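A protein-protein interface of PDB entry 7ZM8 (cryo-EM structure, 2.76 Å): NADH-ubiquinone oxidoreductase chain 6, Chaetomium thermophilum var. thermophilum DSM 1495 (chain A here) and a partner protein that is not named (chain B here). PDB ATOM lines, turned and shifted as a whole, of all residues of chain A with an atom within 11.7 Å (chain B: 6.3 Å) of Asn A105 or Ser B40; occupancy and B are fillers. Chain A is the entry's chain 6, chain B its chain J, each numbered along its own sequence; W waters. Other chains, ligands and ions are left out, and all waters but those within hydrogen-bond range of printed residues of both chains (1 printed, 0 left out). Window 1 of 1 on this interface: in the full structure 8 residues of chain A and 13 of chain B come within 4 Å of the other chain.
The side-chain hydroxyl (OG) of Ser B40 sits at hydrogen-bond distance from the side-chain hydroxyl (OG) of Ser A106 (3.2 Å).
ND2 of Asn A105 sits at hydrogen-bond distance from O of Lys B44 (2.6 Å).
The side-chain amide nitrogen (ND2) of Asn B45 is in hydrogen-bond range of the side-chain amide oxygen (OD1) of Asn A102, 2.7 Å away.
The side-chain amide oxygen (OD1) of Asn A105 lies within hydrogen-bond range of the backbone NH (N) of Val B46 (3.4 Å).
The backbone NH (N) of Gly B47 lies within hydrogen-bond range of the side-chain amide oxygen (OD1) of Asn A105, at 2.8 Å.
N of Pro B48 sits close to O of Ser A104 (3.5 Å).
The backbone carbonyl oxygen of Ala B35 lies within hydrogen-bond range of the side-chain hydroxyl of Thr B39.
The side-chain hydroxyl of Thr B39 lies within hydrogen-bond range of the side-chain amide oxygen of Asn B55 (3.1 Å).
O of Ser A106 sits at hydrogen-bond distance from OG1 of Thr A110 (2.6 Å).
C of Lys B44 touches ND2 of Asn A102, at 3.6 Å.
Ser A104 touches Gly B47 (OG to CA, 3.7 Å).
CB of Asn A105 touches O of Thr B39, 3.2 Å away.
ND2 of Asn A105 touches O of Ala B42, 3.7 Å away.
Asn A105 touches Asn B45.
Pro B48 touches Pro A108.
CB of Ala B36 touches CD1 of Leu A109, 3.5 Å away.
CA of Val B37 touches CD2 of Leu A109, 3.9 Å away.
CD2 of Leu A109 touches CB of Ser B40, at 3.9 Å.
Leu A112 touches Ala B36 (CD1 to CB, 3.8 Å).
Ser A101 touches none of the printed residues of chain B.
Thr A103 touches none of the printed residues of chain B.
Printed residues of chain B within 4 Å of Asn A105: Thr B39 (3.2 Å), Ser B40 (3.5 Å), Ala B42 (3.7 Å), Lys B44 (2.6 Å), Asn B45 (3.997 Å), Val B46 (3.4 Å) and Gly B47 (2.8 Å).
Printed residues of chain B within 4 Å of Leu A109: Ala B36, Val B37 and Ser B40.
Of chain A, only Leu A109 and Leu A112 come within 4 Å of Ala B36.
Val B37 touches just one residue of chain A: Leu A109 (3.9 Å).
Of chain A, only Asn A105, Ser A106 and Leu A109 come within 4 Å of Ser B40.
No residue of chain A comes within 4 Å of Leu B41.
Of chain A, only Asn A105 comes within 4 Å of Ala B42.
Printed residues of chain A within 4 Å of Lys B44: Asn A102 (3.6 Å) and Asn A105 (2.6 Å).
Val B46 touches just one residue of chain A: Asn A105.
Gly B47 touches just these residues of chain A: Ser A104 (3.7 Å) and Asn A105 (2.8 Å).
Pro B48 touches just these residues of chain A: Ser A104 and Pro A108.
Of the 15 printed residues of chain A, 7 touch a printed residue of chain B.
Hydrophobic or aromatic side chains of chain A within 4 Å of the printed part of chain B: Pro A108, Leu A109 and Leu A112.
Of the 15 printed residues of chain B, 10 touch a printed residue of chain A.
Printed residues of chain B that touch a printed residue of chain A: Ala B36, Val B37, Thr B39, Ser B40, Ala B42, Lys B44, Asn B45, Val B46, Gly B47 and Pro B48.
Hydrophobic or aromatic side chains of chain B that line the printed part of chain A: Ala B36, Val B46 and Pro B48.
Water W1 lies within hydrogen-bond range of O of Asn A105 (2.8 Å), O of Ala B36 (2.8 Å) and N of Leu A109 (3.0 Å).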
ATOM      1  N   GLN A 100      16.698 -32.592   0.568  1.00  0.00           N
ATOM      2  CA  GLN A 100      16.896 -32.179   1.945  1.00  0.00           C
ATOM      3  C   GLN A 100      18.373 -31.907   2.187  1.00  0.00           C
ATOM      4  O   GLN A 100      19.226 -32.727   1.832  1.00  0.00           O
ATOM      5  CB  GLN A 100      16.390 -33.251   2.911  1.00  0.00           C
ATOM      6  CG  GLN A 100      16.514 -32.873   4.373  1.00  0.00           C
ATOM      7  CD  GLN A 100      15.828 -31.563   4.690  1.00  0.00           C
ATOM      8  OE1 GLN A 100      14.740 -31.282   4.190  1.00  0.00           O
ATOM      9  NE2 GLN A 100      16.466 -30.749   5.522  1.00  0.00           N
ATOM     10  N   SER A 101      18.666 -30.758   2.782  1.00  0.00           N
ATOM     11  CA  SER A 101      20.021 -30.369   3.132  1.00  0.00           C
ATOM     12  C   SER A 101      20.090 -30.076   4.624  1.00  0.00           C
ATOM     13  O   SER A 101      19.077 -29.833   5.283  1.00  0.00           O
ATOM     14  CB  SER A 101      20.471 -29.150   2.321  1.00  0.00           C
ATOM     15  OG  SER A 101      19.774 -27.986   2.726  1.00  0.00           O
ATOM     16  N   ASN A 102      21.308 -30.099   5.157  1.00  0.00           N
ATOM     17  CA  ASN A 102      21.524 -29.865   6.583  1.00  0.00           C
ATOM     18  C   ASN A 102      21.285 -28.393   6.873  1.00  0.00           C
ATOM     19  O   ASN A 102      22.196 -27.572   6.773  1.00  0.00           O
ATOM     20  CB  ASN A 102      22.931 -30.285   6.985  1.00  0.00           C
ATOM     21  CG  ASN A 102      23.163 -31.774   6.817  1.00  0.00           C
ATOM     22  OD1 ASN A 102      22.386 -32.593   7.308  1.00  0.00           O
ATOM     23  ND2 ASN A 102      24.230 -32.130   6.114  1.00  0.00           N
ATOM     24  N   THR A 103      20.046 -28.057   7.241  1.00  0.00           N
ATOM     25  CA  THR A 103      19.679 -26.661   7.448  1.00  0.00           C
ATOM     26  C   THR A 103      20.402 -26.050   8.639  1.00  0.00           C
ATOM     27  O   THR A 103      20.564 -24.827   8.699  1.00  0.00           O
ATOM     28  CB  THR A 103      18.169 -26.539   7.640  1.00  0.00           C
ATOM     29  OG1 THR A 103      17.785 -27.224   8.838  1.00  0.00           O
ATOM     30  CG2 THR A 103      17.434 -27.149   6.459  1.00  0.00           C
ATOM     31  N   SER A 104      20.919 -26.876   9.541  1.00  0.00           N
ATOM     32  CA  SER A 104      21.543 -26.333  10.766  1.00  0.00           C
ATOM     33  C   SER A 104      22.882 -25.697  10.407  1.00  0.00           C
ATOM     34  O   SER A 104      23.253 -24.719  11.055  1.00  0.00           O
ATOM     35  CB  SER A 104      21.667 -27.415  11.781  1.00  0.00           C
ATOM     36  OG  SER A 104      22.265 -28.568  11.209  1.00  0.00           O
ATOM     37  N   ASN A 105      23.555 -26.212   9.383  1.00  0.00           N
ATOM     38  CA  ASN A 105      24.849 -25.670   8.914  1.00  0.00           C
ATOM     39  C   ASN A 105      24.580 -24.238   8.470  1.00  0.00           C
ATOM     40  O   ASN A 105      25.412 -23.366   8.714  1.00  0.00           O
ATOM     41  CB  ASN A 105      25.328 -26.485   7.722  1.00  0.00           C
ATOM     42  CG  ASN A 105      25.432 -27.962   8.006  1.00  0.00           C
ATOM     43  OD1 ASN A 105      25.163 -28.406   9.118  1.00  0.00           O
ATOM     44  ND2 ASN A 105      25.821 -28.728   7.004  1.00  0.00           N
ATOM     45  N   SER A 106      23.401 -24.006   7.894  1.00  0.00           N
ATOM     46  CA  SER A 106      23.049 -22.673   7.345  1.00  0.00           C
ATOM     47  C   SER A 106      22.401 -21.767   8.398  1.00  0.00           C
ATOM     48  O   SER A 106      22.135 -20.605   8.064  1.00  0.00           O
ATOM     49  CB  SER A 106      22.140 -22.874   6.184  1.00  0.00           C
ATOM     50  OG  SER A 106      22.538 -24.010   5.434  1.00  0.00           O
ATOM     51  N   ILE A 107      22.174 -22.260   9.615  1.00  0.00           N
ATOM     52  CA  ILE A 107      21.468 -21.466  10.671  1.00  0.00           C
ATOM     53  C   ILE A 107      22.245 -20.214  11.119  1.00  0.00           C
ATOM     54  O   ILE A 107      21.598 -19.175  11.300  1.00  0.00           O
ATOM     55  CB  ILE A 107      21.015 -22.370  11.841  1.00  0.00           C
ATOM     56  CG1 ILE A 107      19.751 -23.155  11.482  1.00  0.00           C
ATOM     57  CG2 ILE A 107      20.824 -21.577  13.125  1.00  0.00           C
ATOM     58  CD1 ILE A 107      18.610 -22.287  11.004  1.00  0.00           C
ATOM     59  N   PRO A 108      23.580 -20.229  11.320  1.00  0.00           N
ATOM     60  CA  PRO A 108      24.302 -19.018  11.673  1.00  0.00           C
ATOM     61  C   PRO A 108      24.174 -17.896  10.637  1.00  0.00           C
ATOM     62  O   PRO A 108      24.061 -16.759  11.051  1.00  0.00           O
ATOM     63  CB  PRO A 108      25.763 -19.466  11.624  1.00  0.00           C
ATOM     64  CG  PRO A 108      25.713 -20.909  12.029  1.00  0.00           C
ATOM     65  CD  PRO A 108      24.446 -21.414  11.379  1.00  0.00           C
ATOM     66  N   LEU A 109      24.207 -18.224   9.344  1.00  0.00           N
ATOM     67  CA  LEU A 109      24.144 -17.204   8.271  1.00  0.00           C
ATOM     68  C   LEU A 109      22.725 -16.666   8.205  1.00  0.00           C
ATOM     69  O   LEU A 109      22.523 -15.623   7.594  1.00  0.00           O
ATOM     70  CB  LEU A 109      24.558 -17.848   6.947  1.00  0.00           C
ATOM     71  CG  LEU A 109      24.825 -16.905   5.775  1.00  0.00           C
ATOM     72  CD1 LEU A 109      25.826 -15.828   6.154  1.00  0.00           C
ATOM     73  CD2 LEU A 109      25.317 -17.683   4.566  1.00  0.00           C
ATOM     74  N   THR A 110      21.788 -17.332   8.857  1.00  0.00           N
ATOM     75  CA  THR A 110      20.368 -16.931   8.775  1.00  0.00           C
ATOM     76  C   THR A 110      20.182 -15.828   9.810  1.00  0.00           C
ATOM     77  O   THR A 110      19.443 -14.874   9.518  1.00  0.00           O
ATOM     78  CB  THR A 110      19.468 -18.153   8.971  1.00  0.00           C
ATOM     79  OG1 THR A 110      19.973 -19.192   8.135  1.00  0.00           O
ATOM     80  CG2 THR A 110      18.018 -17.882   8.637  1.00  0.00           C
ATOM     81  N   ILE A 111      20.848 -15.937  10.957  1.00  0.00           N
ATOM     82  CA  ILE A 111      20.807 -14.832  11.911  1.00  0.00           C
ATOM     83  C   ILE A 111      21.509 -13.609  11.339  1.00  0.00           C
ATOM     84  O   ILE A 111      21.028 -12.478  11.471  1.00  0.00           O
ATOM     85  CB  ILE A 111      21.426 -15.265  13.253  1.00  0.00           C
ATOM     86  CG1 ILE A 111      20.579 -16.357  13.904  1.00  0.00           C
ATOM     87  CG2 ILE A 111      21.567 -14.076  14.186  1.00  0.00           C
ATOM     88  CD1 ILE A 111      21.281 -17.080  15.028  1.00  0.00           C
ATOM     89  N   LEU A 112      22.657 -13.818  10.691  1.00  0.00           N
ATOM     90  CA  LEU A 112      23.421 -12.699  10.153  1.00  0.00           C
ATOM     91  C   LEU A 112      22.650 -11.974   9.058  1.00  0.00           C
ATOM     92  O   LEU A 112      22.481 -10.751   9.109  1.00  0.00           O
ATOM     93  CB  LEU A 112      24.759 -13.198   9.617  1.00  0.00           C
ATOM     94  CG  LEU A 112      25.773 -13.652  10.663  1.00  0.00           C
ATOM     95  CD1 LEU A 112      27.113 -13.883   9.997  1.00  0.00           C
ATOM     96  CD2 LEU A 112      25.889 -12.632  11.784  1.00  0.00           C
ATOM     97  N   VAL A 113      22.172 -12.716   8.059  1.00  0.00           N
ATOM     98  CA  VAL A 113      21.531 -12.084   6.911  1.00  0.00           C
ATOM     99  C   VAL A 113      20.225 -11.420   7.323  1.00  0.00           C
ATOM    100  O   VAL A 113      19.889 -10.330   6.846  1.00  0.00           O
ATOM    101  CB  VAL A 113      21.320 -13.114   5.787  1.00  0.00           C
ATOM    102  CG1 VAL A 113      20.549 -12.497   4.635  1.00  0.00           C
ATOM    103  CG2 VAL A 113      22.658 -13.647   5.307  1.00  0.00           C
ATOM    104  N   GLY A 114      19.470 -12.059   8.218  1.00  0.00           N
ATOM    105  CA  GLY A 114      18.213 -11.478   8.657  1.00  0.00           C
ATOM    106  C   GLY A 114      18.394 -10.165   9.395  1.00  0.00           C
ATOM    107  O   GLY A 114      17.610  -9.229   9.219  1.00  0.00           O
ATOM    108  N   ALA B  35      32.916 -16.700   7.531  1.00  0.00           N
ATOM    109  CA  ALA B  35      32.899 -18.019   8.203  1.00  0.00           C
ATOM    110  C   ALA B  35      31.511 -18.635   8.079  1.00  0.00           C
ATOM    111  O   ALA B  35      31.421 -19.866   7.971  1.00  0.00           O
ATOM    112  CB  ALA B  35      33.283 -17.836   9.643  1.00  0.00           C
ATOM    113  N   ALA B  36      30.472 -17.804   8.180  1.00  0.00           N
ATOM    114  CA  ALA B  36      29.076 -18.286   8.119  1.00  0.00           C
ATOM    115  C   ALA B  36      28.761 -18.901   6.754  1.00  0.00           C
ATOM    116  O   ALA B  36      28.016 -19.868   6.710  1.00  0.00           O
ATOM    117  CB  ALA B  36      28.151 -17.162   8.465  1.00  0.00           C
ATOM    118  N   VAL B  37      29.275 -18.318   5.682  1.00  0.00           N
ATOM    119  CA  VAL B  37      29.078 -18.860   4.310  1.00  0.00           C
ATOM    120  C   VAL B  37      29.721 -20.239   4.266  1.00  0.00           C
ATOM    121  O   VAL B  37      29.154 -21.129   3.629  1.00  0.00           O
ATOM    122  CB  VAL B  37      29.710 -17.909   3.281  1.00  0.00           C
ATOM    123  CG1 VAL B  37      29.487 -18.380   1.853  1.00  0.00           C
ATOM    124  CG2 VAL B  37      29.195 -16.494   3.456  1.00  0.00           C
ATOM    125  N   ARG B  38      30.870 -20.392   4.922  1.00  0.00           N
ATOM    126  CA  ARG B  38      31.611 -21.674   4.930  1.00  0.00           C
ATOM    127  C   ARG B  38      30.758 -22.739   5.608  1.00  0.00           C
ATOM    128  O   ARG B  38      30.773 -23.882   5.150  1.00  0.00           O
ATOM    129  CB  ARG B  38      32.935 -21.435   5.649  1.00  0.00           C
ATOM    130  CG  ARG B  38      33.966 -20.684   4.822  1.00  0.00           C
ATOM    131  CD  ARG B  38      34.706 -21.634   3.903  1.00  0.00           C
ATOM    132  NE  ARG B  38      35.382 -22.680   4.657  1.00  0.00           N
ATOM    133  CZ  ARG B  38      36.648 -22.623   5.053  1.00  0.00           C
ATOM    134  NH1 ARG B  38      37.388 -21.570   4.759  1.00  0.00           N
ATOM    135  NH2 ARG B  38      37.172 -23.625   5.738  1.00  0.00           N
ATOM    136  N   THR B  39      30.088 -22.368   6.692  1.00  0.00           N
ATOM    137  CA  THR B  39      29.205 -23.296   7.430  1.00  0.00           C
ATOM    138  C   THR B  39      28.020 -23.660   6.545  1.00  0.00           C
ATOM    139  O   THR B  39      27.733 -24.855   6.420  1.00  0.00           O
ATOM    140  CB  THR B  39      28.779 -22.643   8.746  1.00  0.00           C
ATOM    141  OG1 THR B  39      29.857 -21.822   9.195  1.00  0.00           O
ATOM    142  CG2 THR B  39      28.416 -23.647   9.818  1.00  0.00           C
ATOM    143  N   SER B  40      27.420 -22.665   5.899  1.00  0.00           N
ATOM    144  CA  SER B  40      26.240 -22.894   5.025  1.00  0.00           C
ATOM    145  C   SER B  40      26.623 -23.777   3.849  1.00  0.00           C
ATOM    146  O   SER B  40      25.784 -24.592   3.438  1.00  0.00           O
ATOM    147  CB  SER B  40      25.683 -21.602   4.550  1.00  0.00           C
ATOM    148  OG  SER B  40      24.358 -21.771   4.074  1.00  0.00           O
ATOM    149  N   LEU B  41      27.828 -23.588   3.315  1.00  0.00           N
ATOM    150  CA  LEU B  41      28.252 -24.338   2.112  1.00  0.00           C
ATOM    151  C   LEU B  41      28.883 -25.677   2.482  1.00  0.00           C
ATOM    152  O   LEU B  41      29.167 -26.443   1.555  1.00  0.00           O
ATOM    153  CB  LEU B  41      29.180 -23.464   1.273  1.00  0.00           C
ATOM    154  CG  LEU B  41      28.464 -22.408   0.436  1.00  0.00           C
ATOM    155  CD1 LEU B  41      29.421 -21.752  -0.543  1.00  0.00           C
ATOM    156  CD2 LEU B  41      27.282 -23.021  -0.295  1.00  0.00           C
ATOM    157  N   ALA B  42      29.051 -25.967   3.772  1.00  0.00           N
ATOM    158  CA  ALA B  42      29.706 -27.213   4.140  1.00  0.00           C
ATOM    159  C   ALA B  42      28.875 -28.401   3.677  1.00  0.00           C
ATOM    160  O   ALA B  42      27.646 -28.402   3.780  1.00  0.00           O
ATOM    161  CB  ALA B  42      29.921 -27.274   5.651  1.00  0.00           C
ATOM    162  N   ARG B  43      29.557 -29.421   3.168  1.00  0.00           N
ATOM    163  CA  ARG B  43      28.903 -30.551   2.525  1.00  0.00           C
ATOM    164  C   ARG B  43      28.566 -31.681   3.489  1.00  0.00           C
ATOM    165  O   ARG B  43      28.047 -32.712   3.050  1.00  0.00           O
ATOM    166  CB  ARG B  43      29.787 -31.079   1.394  1.00  0.00           C
ATOM    167  CG  ARG B  43      30.201 -30.001   0.405  1.00  0.00           C
ATOM    168  CD  ARG B  43      31.026 -30.558  -0.743  1.00  0.00           C
ATOM    169  NE  ARG B  43      31.643 -29.489  -1.523  1.00  0.00           N
ATOM    170  CZ  ARG B  43      31.027 -28.817  -2.492  1.00  0.00           C
ATOM    171  NH1 ARG B  43      31.667 -27.858  -3.146  1.00  0.00           N
ATOM    172  NH2 ARG B  43      29.772 -29.104  -2.806  1.00  0.00           N
ATOM    173  N   LYS B  44      28.848 -31.521   4.777  1.00  0.00           N
ATOM    174  CA  LYS B  44      28.529 -32.522   5.784  1.00  0.00           C
ATOM    175  C   LYS B  44      27.703 -31.890   6.898  1.00  0.00           C
ATOM    176  O   LYS B  44      27.603 -30.666   7.016  1.00  0.00           O
ATOM    177  CB  LYS B  44      29.801 -33.157   6.356  1.00  0.00           C
ATOM    178  CG  LYS B  44      30.529 -34.066   5.381  1.00  0.00           C
ATOM    179  CD  LYS B  44      31.740 -34.713   6.029  1.00  0.00           C
ATOM    180  CE  LYS B  44      31.321 -35.741   7.064  1.00  0.00           C
ATOM    181  NZ  LYS B  44      30.630 -36.904   6.441  1.00  0.00           N
ATOM    182  N   ASN B  45      27.107 -32.751   7.725  1.00  0.00           N
ATOM    183  CA  ASN B  45      26.249 -32.309   8.825  1.00  0.00           C
ATOM    184  C   ASN B  45      27.119 -31.786   9.968  1.00  0.00           C
ATOM    185  O   ASN B  45      27.280 -32.409  11.020  1.00  0.00           O
ATOM    186  CB  ASN B  45      25.344 -33.446   9.280  1.00  0.00           C
ATOM    187  CG  ASN B  45      24.144 -32.957  10.068  1.00  0.00           C
ATOM    188  OD1 ASN B  45      24.268 -32.105  10.946  1.00  0.00           O
ATOM    189  ND2 ASN B  45      22.973 -33.498   9.756  1.00  0.00           N
ATOM    190  N   VAL B  46      27.688 -30.601   9.742  1.00  0.00           N
ATOM    191  CA  VAL B  46      28.555 -29.989  10.740  1.00  0.00           C
ATOM    192  C   VAL B  46      27.774 -29.226  11.802  1.00  0.00           C
ATOM    193  O   VAL B  46      28.323 -28.933  12.869  1.00  0.00           O
ATOM    194  CB  VAL B  46      29.575 -29.059  10.065  1.00  0.00           C
ATOM    195  CG1 VAL B  46      30.467 -29.853   9.128  1.00  0.00           C
ATOM    196  CG2 VAL B  46      28.853 -27.962   9.302  1.00  0.00           C
ATOM    197  N   GLY B  47      26.513 -28.895  11.539  1.00  0.00           N
ATOM    198  CA  GLY B  47      25.675 -28.248  12.520  1.00  0.00           C
ATOM    199  C   GLY B  47      25.916 -26.758  12.624  1.00  0.00           C
ATOM    200  O   GLY B  47      26.712 -26.176  11.882  1.00  0.00           O
ATOM    201  N   PRO B  48      25.220 -26.108  13.559  1.00  0.00           N
ATOM    202  CA  PRO B  48      25.372 -24.653  13.698  1.00  0.00           C
ATOM    203  C   PRO B  48      26.667 -24.237  14.371  1.00  0.00           C
ATOM    204  O   PRO B  48      27.233 -23.202  14.005  1.00  0.00           O
ATOM    205  CB  PRO B  48      24.151 -24.247  14.536  1.00  0.00           C
ATOM    206  CG  PRO B  48      23.272 -25.472  14.607  1.00  0.00           C
ATOM    207  CD  PRO B  48      24.182 -26.639  14.451  1.00  0.00           C
ATOM    208  N   ASN B  55      35.420 -23.078  11.349  1.00  0.00           N
ATOM    209  CA  ASN B  55      35.691 -21.826  10.654  1.00  0.00           C
ATOM    210  C   ASN B  55      36.043 -20.691  11.606  1.00  0.00           C
ATOM    211  O   ASN B  55      36.120 -19.538  11.173  1.00  0.00           O
ATOM    212  CB  ASN B  55      34.493 -21.421   9.793  1.00  0.00           C
ATOM    213  CG  ASN B  55      33.979 -22.554   8.942  1.00  0.00           C
ATOM    214  OD1 ASN B  55      32.801 -22.898   8.995  1.00  0.00           O
ATOM    215  ND2 ASN B  55      34.859 -23.137   8.143  1.00  0.00           N
HETATM  216  O   HOH W   1      25.814 -20.587   8.342  1.00  0.00           O
